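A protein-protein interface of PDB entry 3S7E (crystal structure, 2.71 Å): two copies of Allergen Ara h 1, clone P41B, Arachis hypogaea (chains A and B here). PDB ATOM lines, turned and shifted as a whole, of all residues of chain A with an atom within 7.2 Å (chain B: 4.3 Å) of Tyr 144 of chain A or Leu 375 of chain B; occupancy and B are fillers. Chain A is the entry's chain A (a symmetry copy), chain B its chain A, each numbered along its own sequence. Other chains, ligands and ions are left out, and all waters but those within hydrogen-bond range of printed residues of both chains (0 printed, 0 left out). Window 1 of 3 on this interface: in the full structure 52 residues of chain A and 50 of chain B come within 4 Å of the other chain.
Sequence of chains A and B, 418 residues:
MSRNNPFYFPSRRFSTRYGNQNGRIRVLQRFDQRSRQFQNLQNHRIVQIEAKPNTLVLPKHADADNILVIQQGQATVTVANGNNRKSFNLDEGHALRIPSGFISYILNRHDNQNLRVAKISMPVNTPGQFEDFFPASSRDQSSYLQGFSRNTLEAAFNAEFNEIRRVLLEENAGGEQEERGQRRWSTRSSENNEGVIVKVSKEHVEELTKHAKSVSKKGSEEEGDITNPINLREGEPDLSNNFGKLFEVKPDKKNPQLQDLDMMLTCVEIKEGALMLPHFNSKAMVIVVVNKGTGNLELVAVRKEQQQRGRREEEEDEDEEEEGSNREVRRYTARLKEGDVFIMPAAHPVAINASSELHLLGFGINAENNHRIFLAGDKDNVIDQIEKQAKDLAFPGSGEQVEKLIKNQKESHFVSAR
The side-chain hydroxyl (OG) of Ser 142 of chain A sits at hydrogen-bond distance from the side-chain amide oxygen (OE1) of Gln 146 of chain A (2.7 Å).
N of Tyr 144 of chain A sits close to O of Phe 134 of chain A (3.2 Å).
The backbone carbonyl oxygen (O) of Pro 278 of chain B sits at hydrogen-bond distance from the backbone NH (N) of Leu 375 of chain B (3.2 Å).
OG of Ser 137 of chain A is in hydrogen-bond range of N of Ser 143 of chain A, at 2.9 Å.
N of Val 300 of chain B lies within hydrogen-bond range of O of Pro 349 of chain B, 3.1 Å away.
The backbone carbonyl oxygen (O) of Phe 374 of chain B lies within hydrogen-bond range of the backbone NH (N) of Val 382 of chain B (2.8 Å).
Among the printed residues, pairs that only touch across the chains: His 61 of chain A with Phe 280 of chain B (3.0 Å), Tyr 144 of chain A with Leu 375 of chain B (3.3 Å), Phe 148 of chain A with Val 300 of chain B (3.3 Å), Gly 147 of chain A with Val 300 of chain B (3.4 Å), Tyr 144 of chain A with Val 300 of chain B (3.4 Å), Ser 143 of chain A with Val 329 of chain B (3.5 Å), Phe 148 of chain A with Pro 278 of chain B (3.6 Å), Phe 133 of chain A with Pro 349 of chain B (3.6 Å), Ser 142 of chain A with Val 329 of chain B (3.7 Å), Tyr 144 of chain A with Pro 349 of chain B (3.8 Å), Ala 156 of chain A with Pro 278 of chain B (3.8 Å), Tyr 144 of chain A with Val 329 of chain B (3.8 Å), Gly 147 of chain A with Val 329 of chain B (3.9 Å), Ile 103 of chain A with Val 382 of chain B (3.9 Å), Phe 157 of chain A with Leu 375 of chain B (3.96 Å) and Phe 148 of chain A with Pro 349 of chain B (3.99 Å).
Of chain B, only Val 300, Val 329, Pro 349 and Leu 375 come within 4 Å of Tyr 144 of chain A.
Of chain A, only Tyr 144 and Phe 157 come within 4 Å of Leu 375 of chain B.
Of the printed residues of chain B, Ile 103 of chain A touches Val 382 (3.9 Å).
Of the printed residues of chain A, Pro 349 of chain B touches Phe 133, Tyr 144 and Phe 148.
Of the printed residues of chain A, Val 300 of chain B touches Tyr 144, Gly 147 and Phe 148.
Of the printed residues of chain B, Gly 147 of chain A touches Val 300 (3.4 Å) and Val 329 (3.9 Å).
Gln 146 of chain A touches none of the printed residues of chain B.
The nearest residue of chain A that does not touch Leu 375 of chain B is Leu 145 of chain A (4.7 Å).
No position is printed for both chains.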
ATOM      1  N   PRO A  59     -13.430  28.694 -22.965  1.00  0.00           N
ATOM      2  CA  PRO A  59     -12.510  29.641 -23.553  1.00  0.00           C
ATOM      3  C   PRO A  59     -12.120  29.417 -25.002  1.00  0.00           C
ATOM      4  O   PRO A  59     -11.848  28.285 -25.425  1.00  0.00           O
ATOM      5  CB  PRO A  59     -11.241  29.413 -22.746  1.00  0.00           C
ATOM      6  CG  PRO A  59     -11.737  29.119 -21.407  1.00  0.00           C
ATOM      7  CD  PRO A  59     -12.970  28.284 -21.627  1.00  0.00           C
ATOM      8  N   LYS A  60     -12.115  30.522 -25.736  1.00  0.00           N
ATOM      9  CA  LYS A  60     -11.576  30.593 -27.086  1.00  0.00           C
ATOM     10  C   LYS A  60     -11.586  32.026 -27.571  1.00  0.00           C
ATOM     11  O   LYS A  60     -12.158  32.919 -26.924  1.00  0.00           O
ATOM     12  CB  LYS A  60     -12.457  29.781 -28.036  1.00  0.00           C
ATOM     13  CG  LYS A  60     -13.928  30.104 -27.903  1.00  0.00           C
ATOM     14  CD  LYS A  60     -14.626  30.075 -29.231  1.00  0.00           C
ATOM     15  CE  LYS A  60     -16.109  30.285 -29.037  1.00  0.00           C
ATOM     16  NZ  LYS A  60     -16.395  31.457 -28.167  1.00  0.00           N
ATOM     17  N   HIS A  61     -10.958  32.216 -28.722  1.00  0.00           N
ATOM     18  CA  HIS A  61     -11.082  33.441 -29.479  1.00  0.00           C
ATOM     19  C   HIS A  61     -11.196  33.135 -30.954  1.00  0.00           C
ATOM     20  O   HIS A  61     -10.925  32.025 -31.391  1.00  0.00           O
ATOM     21  CB  HIS A  61      -9.908  34.362 -29.220  1.00  0.00           C
ATOM     22  CG  HIS A  61      -8.588  33.842 -29.706  1.00  0.00           C
ATOM     23  ND1 HIS A  61      -8.458  32.787 -30.580  1.00  0.00           N
ATOM     24  CD2 HIS A  61      -7.332  34.277 -29.459  1.00  0.00           C
ATOM     25  CE1 HIS A  61      -7.175  32.583 -30.831  1.00  0.00           C
ATOM     26  NE2 HIS A  61      -6.472  33.476 -30.167  1.00  0.00           N
ATOM     27  N   ILE A 103      -9.761  36.492 -25.698  1.00  0.00           N
ATOM     28  CA  ILE A 103     -10.386  35.302 -25.144  1.00  0.00           C
ATOM     29  C   ILE A 103     -11.679  35.636 -24.411  1.00  0.00           C
ATOM     30  O   ILE A 103     -11.781  36.656 -23.731  1.00  0.00           O
ATOM     31  CB  ILE A 103      -9.436  34.580 -24.191  1.00  0.00           C
ATOM     32  CG1 ILE A 103      -8.449  33.734 -24.995  1.00  0.00           C
ATOM     33  CG2 ILE A 103     -10.198  33.702 -23.225  1.00  0.00           C
ATOM     34  CD1 ILE A 103      -7.675  32.718 -24.146  1.00  0.00           C
ATOM     35  N   ASP A 132     -12.758  29.392 -34.642  1.00  0.00           N
ATOM     36  CA  ASP A 132     -12.463  29.476 -33.222  1.00  0.00           C
ATOM     37  C   ASP A 132     -11.102  28.858 -32.948  1.00  0.00           C
ATOM     38  O   ASP A 132     -10.675  27.929 -33.630  1.00  0.00           O
ATOM     39  CB  ASP A 132     -13.531  28.762 -32.399  1.00  0.00           C
ATOM     40  CG  ASP A 132     -14.927  29.380 -32.570  1.00  0.00           C
ATOM     41  OD1 ASP A 132     -15.883  28.854 -31.955  1.00  0.00           O
ATOM     42  OD2 ASP A 132     -15.076  30.378 -33.314  1.00  0.00           O
ATOM     43  N   PHE A 133     -10.437  29.405 -31.941  1.00  0.00           N
ATOM     44  CA  PHE A 133      -9.177  28.896 -31.422  1.00  0.00           C
ATOM     45  C   PHE A 133      -9.300  28.588 -29.930  1.00  0.00           C
ATOM     46  O   PHE A 133      -9.341  29.508 -29.104  1.00  0.00           O
ATOM     47  CB  PHE A 133      -8.109  29.950 -31.579  1.00  0.00           C
ATOM     48  CG  PHE A 133      -7.685  30.191 -32.995  1.00  0.00           C
ATOM     49  CD1 PHE A 133      -8.492  30.887 -33.867  1.00  0.00           C
ATOM     50  CD2 PHE A 133      -6.450  29.750 -33.432  1.00  0.00           C
ATOM     51  CE1 PHE A 133      -8.094  31.114 -35.149  1.00  0.00           C
ATOM     52  CE2 PHE A 133      -6.047  29.974 -34.717  1.00  0.00           C
ATOM     53  CZ  PHE A 133      -6.865  30.657 -35.578  1.00  0.00           C
ATOM     54  N   PHE A 134      -9.340  27.304 -29.582  1.00  0.00           N
ATOM     55  CA  PHE A 134      -9.468  26.889 -28.178  1.00  0.00           C
ATOM     56  C   PHE A 134      -8.104  26.564 -27.601  1.00  0.00           C
ATOM     57  O   PHE A 134      -7.381  25.768 -28.179  1.00  0.00           O
ATOM     58  CB  PHE A 134     -10.325  25.638 -28.040  1.00  0.00           C
ATOM     59  CG  PHE A 134     -11.742  25.819 -28.451  1.00  0.00           C
ATOM     60  CD1 PHE A 134     -12.091  25.817 -29.792  1.00  0.00           C
ATOM     61  CD2 PHE A 134     -12.741  25.950 -27.498  1.00  0.00           C
ATOM     62  CE1 PHE A 134     -13.419  25.954 -30.176  1.00  0.00           C
ATOM     63  CE2 PHE A 134     -14.070  26.087 -27.877  1.00  0.00           C
ATOM     64  CZ  PHE A 134     -14.409  26.087 -29.214  1.00  0.00           C
ATOM     65  N   PRO A 135      -7.750  27.155 -26.445  1.00  0.00           N
ATOM     66  CA  PRO A 135      -6.498  26.730 -25.824  1.00  0.00           C
ATOM     67  C   PRO A 135      -6.567  25.282 -25.319  1.00  0.00           C
ATOM     68  O   PRO A 135      -5.550  24.582 -25.316  1.00  0.00           O
ATOM     69  CB  PRO A 135      -6.320  27.716 -24.662  1.00  0.00           C
ATOM     70  CG  PRO A 135      -7.656  28.244 -24.375  1.00  0.00           C
ATOM     71  CD  PRO A 135      -8.445  28.183 -25.646  1.00  0.00           C
ATOM     72  N   ALA A 136      -7.768  24.853 -24.917  1.00  0.00           N
ATOM     73  CA  ALA A 136      -7.998  23.513 -24.381  1.00  0.00           C
ATOM     74  C   ALA A 136      -8.557  22.551 -25.427  1.00  0.00           C
ATOM     75  O   ALA A 136      -9.412  22.923 -26.230  1.00  0.00           O
ATOM     76  CB  ALA A 136      -8.942  23.583 -23.201  1.00  0.00           C
ATOM     77  N   SER A 137      -8.072  21.307 -25.397  1.00  0.00           N
ATOM     78  CA  SER A 137      -8.629  20.222 -26.219  1.00  0.00           C
ATOM     79  C   SER A 137      -9.840  19.611 -25.544  1.00  0.00           C
ATOM     80  O   SER A 137      -9.927  19.591 -24.319  1.00  0.00           O
ATOM     81  CB  SER A 137      -7.616  19.103 -26.428  1.00  0.00           C
ATOM     82  OG  SER A 137      -6.488  19.552 -27.146  1.00  0.00           O
ATOM     83  N   GLN A 141     -13.439  19.325 -30.380  1.00  0.00           N
ATOM     84  CA  GLN A 141     -12.404  20.105 -31.052  1.00  0.00           C
ATOM     85  C   GLN A 141     -11.038  19.815 -30.441  1.00  0.00           C
ATOM     86  O   GLN A 141     -10.910  18.984 -29.551  1.00  0.00           O
ATOM     87  CB  GLN A 141     -12.749  21.608 -31.009  1.00  0.00           C
ATOM     88  CG  GLN A 141     -12.236  22.403 -29.801  1.00  0.00           C
ATOM     89  CD  GLN A 141     -12.285  21.649 -28.499  1.00  0.00           C
ATOM     90  OE1 GLN A 141     -13.290  21.032 -28.166  1.00  0.00           O
ATOM     91  NE2 GLN A 141     -11.192  21.691 -27.755  1.00  0.00           N
ATOM     92  N   SER A 142     -10.027  20.521 -30.928  1.00  0.00           N
ATOM     93  CA  SER A 142      -8.635  20.281 -30.552  1.00  0.00           C
ATOM     94  C   SER A 142      -7.969  21.586 -30.075  1.00  0.00           C
ATOM     95  O   SER A 142      -8.389  22.683 -30.459  1.00  0.00           O
ATOM     96  CB  SER A 142      -7.901  19.682 -31.754  1.00  0.00           C
ATOM     97  OG  SER A 142      -6.580  19.306 -31.422  1.00  0.00           O
ATOM     98  N   SER A 143      -6.952  21.459 -29.222  1.00  0.00           N
ATOM     99  CA  SER A 143      -6.205  22.617 -28.729  1.00  0.00           C
ATOM    100  C   SER A 143      -5.204  23.084 -29.780  1.00  0.00           C
ATOM    101  O   SER A 143      -4.557  22.270 -30.435  1.00  0.00           O
ATOM    102  CB  SER A 143      -5.467  22.292 -27.435  1.00  0.00           C
ATOM    103  OG  SER A 143      -4.585  23.342 -27.064  1.00  0.00           O
ATOM    104  N   TYR A 144      -5.070  24.402 -29.929  1.00  0.00           N
ATOM    105  CA  TYR A 144      -4.158  24.982 -30.932  1.00  0.00           C
ATOM    106  C   TYR A 144      -2.678  24.932 -30.523  1.00  0.00           C
ATOM    107  O   TYR A 144      -1.805  25.320 -31.291  1.00  0.00           O
ATOM    108  CB  TYR A 144      -4.566  26.413 -31.286  1.00  0.00           C
ATOM    109  CG  TYR A 144      -4.620  27.377 -30.129  1.00  0.00           C
ATOM    110  CD1 TYR A 144      -3.458  27.889 -29.555  1.00  0.00           C
ATOM    111  CD2 TYR A 144      -5.842  27.814 -29.628  1.00  0.00           C
ATOM    112  CE1 TYR A 144      -3.519  28.794 -28.496  1.00  0.00           C
ATOM    113  CE2 TYR A 144      -5.908  28.718 -28.571  1.00  0.00           C
ATOM    114  CZ  TYR A 144      -4.748  29.200 -28.013  1.00  0.00           C
ATOM    115  OH  TYR A 144      -4.831  30.089 -26.976  1.00  0.00           O
ATOM    116  N   LEU A 145      -2.417  24.467 -29.306  1.00  0.00           N
ATOM    117  CA  LEU A 145      -1.055  24.225 -28.821  1.00  0.00           C
ATOM    118  C   LEU A 145      -0.555  22.834 -29.195  1.00  0.00           C
ATOM    119  O   LEU A 145       0.649  22.588 -29.165  1.00  0.00           O
ATOM    120  CB  LEU A 145      -0.997  24.378 -27.311  1.00  0.00           C
ATOM    121  CG  LEU A 145      -1.375  25.758 -26.777  1.00  0.00           C
ATOM    122  CD1 LEU A 145      -1.706  25.688 -25.300  1.00  0.00           C
ATOM    123  CD2 LEU A 145      -0.236  26.740 -27.048  1.00  0.00           C
ATOM    124  N   GLN A 146      -1.474  21.930 -29.534  1.00  0.00           N
ATOM    125  CA  GLN A 146      -1.095  20.604 -30.041  1.00  0.00           C
ATOM    126  C   GLN A 146      -0.344  20.683 -31.362  1.00  0.00           C
ATOM    127  O   GLN A 146       0.466  19.816 -31.665  1.00  0.00           O
ATOM    128  CB  GLN A 146      -2.303  19.680 -30.192  1.00  0.00           C
ATOM    129  CG  GLN A 146      -2.562  18.835 -28.962  1.00  0.00           C
ATOM    130  CD  GLN A 146      -3.883  18.080 -29.013  1.00  0.00           C
ATOM    131  OE1 GLN A 146      -4.613  18.135 -30.004  1.00  0.00           O
ATOM    132  NE2 GLN A 146      -4.198  17.365 -27.926  1.00  0.00           N
ATOM    133  N   GLY A 147      -0.611  21.731 -32.134  1.00  0.00           N
ATOM    134  CA  GLY A 147       0.049  21.954 -33.422  1.00  0.00           C
ATOM    135  C   GLY A 147       1.409  22.614 -33.288  1.00  0.00           C
ATOM    136  O   GLY A 147       1.967  23.069 -34.272  1.00  0.00           O
ATOM    137  N   PHE A 148       1.936  22.686 -32.068  1.00  0.00           N
ATOM    138  CA  PHE A 148       3.321  23.123 -31.850  1.00  0.00           C
ATOM    139  C   PHE A 148       4.275  21.925 -31.766  1.00  0.00           C
ATOM    140  O   PHE A 148       3.863  20.785 -31.994  1.00  0.00           O
ATOM    141  CB  PHE A 148       3.402  24.056 -30.637  1.00  0.00           C
ATOM    142  CG  PHE A 148       3.076  25.480 -30.985  1.00  0.00           C
ATOM    143  CD1 PHE A 148       1.779  25.842 -31.291  1.00  0.00           C
ATOM    144  CD2 PHE A 148       4.074  26.436 -31.088  1.00  0.00           C
ATOM    145  CE1 PHE A 148       1.470  27.145 -31.654  1.00  0.00           C
ATOM    146  CE2 PHE A 148       3.769  27.731 -31.452  1.00  0.00           C
ATOM    147  CZ  PHE A 148       2.466  28.087 -31.728  1.00  0.00           C
ATOM    148  N   ALA A 156       9.048  26.892 -24.446  1.00  0.00           N
ATOM    149  CA  ALA A 156       8.087  27.950 -24.122  1.00  0.00           C
ATOM    150  C   ALA A 156       7.654  27.883 -22.664  1.00  0.00           C
ATOM    151  O   ALA A 156       7.810  28.842 -21.904  1.00  0.00           O
ATOM    152  CB  ALA A 156       6.851  27.865 -25.044  1.00  0.00           C
ATOM    153  N   PHE A 157       7.128  26.723 -22.293  1.00  0.00           N
ATOM    154  CA  PHE A 157       6.484  26.528 -20.993  1.00  0.00           C
ATOM    155  C   PHE A 157       7.405  26.154 -19.820  1.00  0.00           C
ATOM    156  O   PHE A 157       6.937  26.109 -18.669  1.00  0.00           O
ATOM    157  CB  PHE A 157       5.429  25.435 -21.114  1.00  0.00           C
ATOM    158  CG  PHE A 157       4.182  25.865 -21.818  1.00  0.00           C
ATOM    159  CD1 PHE A 157       3.056  26.227 -21.098  1.00  0.00           C
ATOM    160  CD2 PHE A 157       4.119  25.882 -23.201  1.00  0.00           C
ATOM    161  CE1 PHE A 157       1.882  26.605 -21.743  1.00  0.00           C
ATOM    162  CE2 PHE A 157       2.951  26.264 -23.859  1.00  0.00           C
ATOM    163  CZ  PHE A 157       1.827  26.625 -23.125  1.00  0.00           C
ATOM    164  N   LEU A 169      -2.905  19.811 -22.587  1.00  0.00           N
ATOM    165  CA  LEU A 169      -3.183  19.359 -23.949  1.00  0.00           C
ATOM    166  C   LEU A 169      -4.203  18.240 -24.138  1.00  0.00           C
ATOM    167  O   LEU A 169      -4.958  18.280 -25.082  1.00  0.00           O
ATOM    168  CB  LEU A 169      -1.875  18.949 -24.618  1.00  0.00           C
ATOM    169  CG  LEU A 169      -0.881  20.053 -24.901  1.00  0.00           C
ATOM    170  CD1 LEU A 169       0.433  19.472 -25.309  1.00  0.00           C
ATOM    171  CD2 LEU A 169      -1.410  20.960 -25.990  1.00  0.00           C
ATOM    172  N   PRO B 278       5.433  31.191 -28.674  1.00  0.00           N
ATOM    173  CA  PRO B 278       4.107  31.161 -29.292  1.00  0.00           C
ATOM    174  C   PRO B 278       3.352  32.444 -28.977  1.00  0.00           C
ATOM    175  O   PRO B 278       3.195  32.812 -27.805  1.00  0.00           O
ATOM    176  CB  PRO B 278       3.435  29.937 -28.655  1.00  0.00           C
ATOM    177  CG  PRO B 278       4.426  29.382 -27.657  1.00  0.00           C
ATOM    178  CD  PRO B 278       5.763  29.905 -28.042  1.00  0.00           C
ATOM    179  N   PHE B 280       0.579  35.756 -31.027  1.00  0.00           N
ATOM    180  CA  PHE B 280      -0.165  36.201 -32.183  1.00  0.00           C
ATOM    181  C   PHE B 280      -0.575  37.644 -32.085  1.00  0.00           C
ATOM    182  O   PHE B 280      -0.341  38.298 -31.086  1.00  0.00           O
ATOM    183  CB  PHE B 280      -1.392  35.328 -32.399  1.00  0.00           C
ATOM    184  CG  PHE B 280      -2.329  35.282 -31.246  1.00  0.00           C
ATOM    185  CD1 PHE B 280      -3.431  36.117 -31.195  1.00  0.00           C
ATOM    186  CD2 PHE B 280      -2.158  34.339 -30.242  1.00  0.00           C
ATOM    187  CE1 PHE B 280      -4.320  36.033 -30.154  1.00  0.00           C
ATOM    188  CE2 PHE B 280      -3.048  34.243 -29.194  1.00  0.00           C
ATOM    189  CZ  PHE B 280      -4.127  35.099 -29.146  1.00  0.00           C
ATOM    190  N   VAL B 300       0.292  28.026 -36.894  1.00  0.00           N
ATOM    191  CA  VAL B 300      -0.810  27.130 -36.515  1.00  0.00           C
ATOM    192  C   VAL B 300      -2.164  27.703 -36.948  1.00  0.00           C
ATOM    193  O   VAL B 300      -2.608  28.753 -36.456  1.00  0.00           O
ATOM    194  CB  VAL B 300      -0.826  26.874 -35.002  1.00  0.00           C
ATOM    195  CG1 VAL B 300      -2.123  26.198 -34.585  1.00  0.00           C
ATOM    196  CG2 VAL B 300       0.379  26.052 -34.608  1.00  0.00           C
ATOM    197  N   VAL B 329      -6.802  21.501 -36.066  1.00  0.00           N
ATOM    198  CA  VAL B 329      -5.602  22.284 -35.770  1.00  0.00           C
ATOM    199  C   VAL B 329      -4.463  21.732 -36.607  1.00  0.00           C
ATOM    200  O   VAL B 329      -3.785  20.791 -36.204  1.00  0.00           O
ATOM    201  CB  VAL B 329      -5.214  22.264 -34.270  1.00  0.00           C
ATOM    202  CG1 VAL B 329      -3.809  22.853 -34.059  1.00  0.00           C
ATOM    203  CG2 VAL B 329      -6.230  23.039 -33.454  1.00  0.00           C
ATOM    204  N   PRO B 349      -1.823  31.664 -33.958  1.00  0.00           N
ATOM    205  CA  PRO B 349      -0.531  31.534 -33.271  1.00  0.00           C
ATOM    206  C   PRO B 349       0.710  31.255 -34.139  1.00  0.00           C
ATOM    207  O   PRO B 349       0.669  30.445 -35.072  1.00  0.00           O
ATOM    208  CB  PRO B 349      -0.777  30.380 -32.306  1.00  0.00           C
ATOM    209  CG  PRO B 349      -2.262  30.504 -31.987  1.00  0.00           C
ATOM    210  CD  PRO B 349      -2.872  30.870 -33.297  1.00  0.00           C
ATOM    211  N   PHE B 374       0.369  36.903 -26.144  1.00  0.00           N
ATOM    212  CA  PHE B 374       1.313  35.804 -25.947  1.00  0.00           C
ATOM    213  C   PHE B 374       0.694  34.672 -25.140  1.00  0.00           C
ATOM    214  O   PHE B 374      -0.109  34.880 -24.230  1.00  0.00           O
ATOM    215  CB  PHE B 374       2.612  36.285 -25.292  1.00  0.00           C
ATOM    216  CG  PHE B 374       3.574  36.938 -26.250  1.00  0.00           C
ATOM    217  CD1 PHE B 374       4.722  36.281 -26.657  1.00  0.00           C
ATOM    218  CD2 PHE B 374       3.336  38.211 -26.727  1.00  0.00           C
ATOM    219  CE1 PHE B 374       5.614  36.885 -27.530  1.00  0.00           C
ATOM    220  CE2 PHE B 374       4.221  38.818 -27.602  1.00  0.00           C
ATOM    221  CZ  PHE B 374       5.358  38.155 -28.008  1.00  0.00           C
ATOM    222  N   LEU B 375       1.087  33.461 -25.501  1.00  0.00           N
ATOM    223  CA  LEU B 375       0.492  32.257 -24.948  1.00  0.00           C
ATOM    224  C   LEU B 375       1.418  31.578 -23.926  1.00  0.00           C
ATOM    225  O   LEU B 375       1.105  30.505 -23.401  1.00  0.00           O
ATOM    226  CB  LEU B 375       0.142  31.325 -26.100  1.00  0.00           C
ATOM    227  CG  LEU B 375      -0.887  31.974 -27.024  1.00  0.00           C
ATOM    228  CD1 LEU B 375      -0.995  31.237 -28.341  1.00  0.00           C
ATOM    229  CD2 LEU B 375      -2.231  32.039 -26.324  1.00  0.00           C
ATOM    230  N   ALA B 376       2.540  32.230 -23.632  1.00  0.00           N
ATOM    231  CA  ALA B 376       3.522  31.715 -22.682  1.00  0.00           C
ATOM    232  C   ALA B 376       4.476  32.814 -22.182  1.00  0.00           C
ATOM    233  O   ALA B 376       4.927  33.663 -22.951  1.00  0.00           O
ATOM    234  CB  ALA B 376       4.304  30.593 -23.314  1.00  0.00           C
ATOM    235  N   ASN B 381       0.946  37.291 -21.142  1.00  0.00           N
ATOM    236  CA  ASN B 381       0.409  35.958 -21.094  1.00  0.00           C
ATOM    237  C   ASN B 381      -1.081  36.096 -21.007  1.00  0.00           C
ATOM    238  O   ASN B 381      -1.601  36.602 -20.020  1.00  0.00           O
ATOM    239  CB  ASN B 381       0.925  35.168 -19.906  1.00  0.00           C
ATOM    240  CG  ASN B 381       0.775  33.669 -20.105  1.00  0.00           C
ATOM    241  OD1 ASN B 381       0.102  33.221 -21.037  1.00  0.00           O
ATOM    242  ND2 ASN B 381       1.405  32.887 -19.230  1.00  0.00           N
ATOM    243  N   VAL B 382      -1.760  35.682 -22.067  1.00  0.00           N
ATOM    244  CA  VAL B 382      -3.218  35.711 -22.111  1.00  0.00           C
ATOM    245  C   VAL B 382      -3.838  34.585 -21.256  1.00  0.00           C
ATOM    246  O   VAL B 382      -4.875  34.790 -20.618  1.00  0.00           O
ATOM    247  CB  VAL B 382      -3.736  35.649 -23.567  1.00  0.00           C
ATOM    248  CG1 VAL B 382      -3.276  34.377 -24.247  1.00  0.00           C
ATOM    249  CG2 VAL B 382      -5.254  35.761 -23.610  1.00  0.00           C
ATOM    250  N   ILE B 383      -3.204  33.413 -21.232  1.00  0.00           N
ATOM    251  CA  ILE B 383      -3.743  32.264 -20.482  1.00  0.00           C
ATOM    252  C   ILE B 383      -3.793  32.540 -18.988  1.00  0.00           C
ATOM    253  O   ILE B 383      -4.797  32.277 -18.342  1.00  0.00           O
ATOM    254  CB  ILE B 383      -2.919  30.980 -20.690  1.00  0.00           C
ATOM    255  CG1 ILE B 383      -2.994  30.537 -22.153  1.00  0.00           C
ATOM    256  CG2 ILE B 383      -3.432  29.863 -19.782  1.00  0.00           C
ATOM    257  CD1 ILE B 383      -2.301  29.218 -22.423  1.00  0.00           C
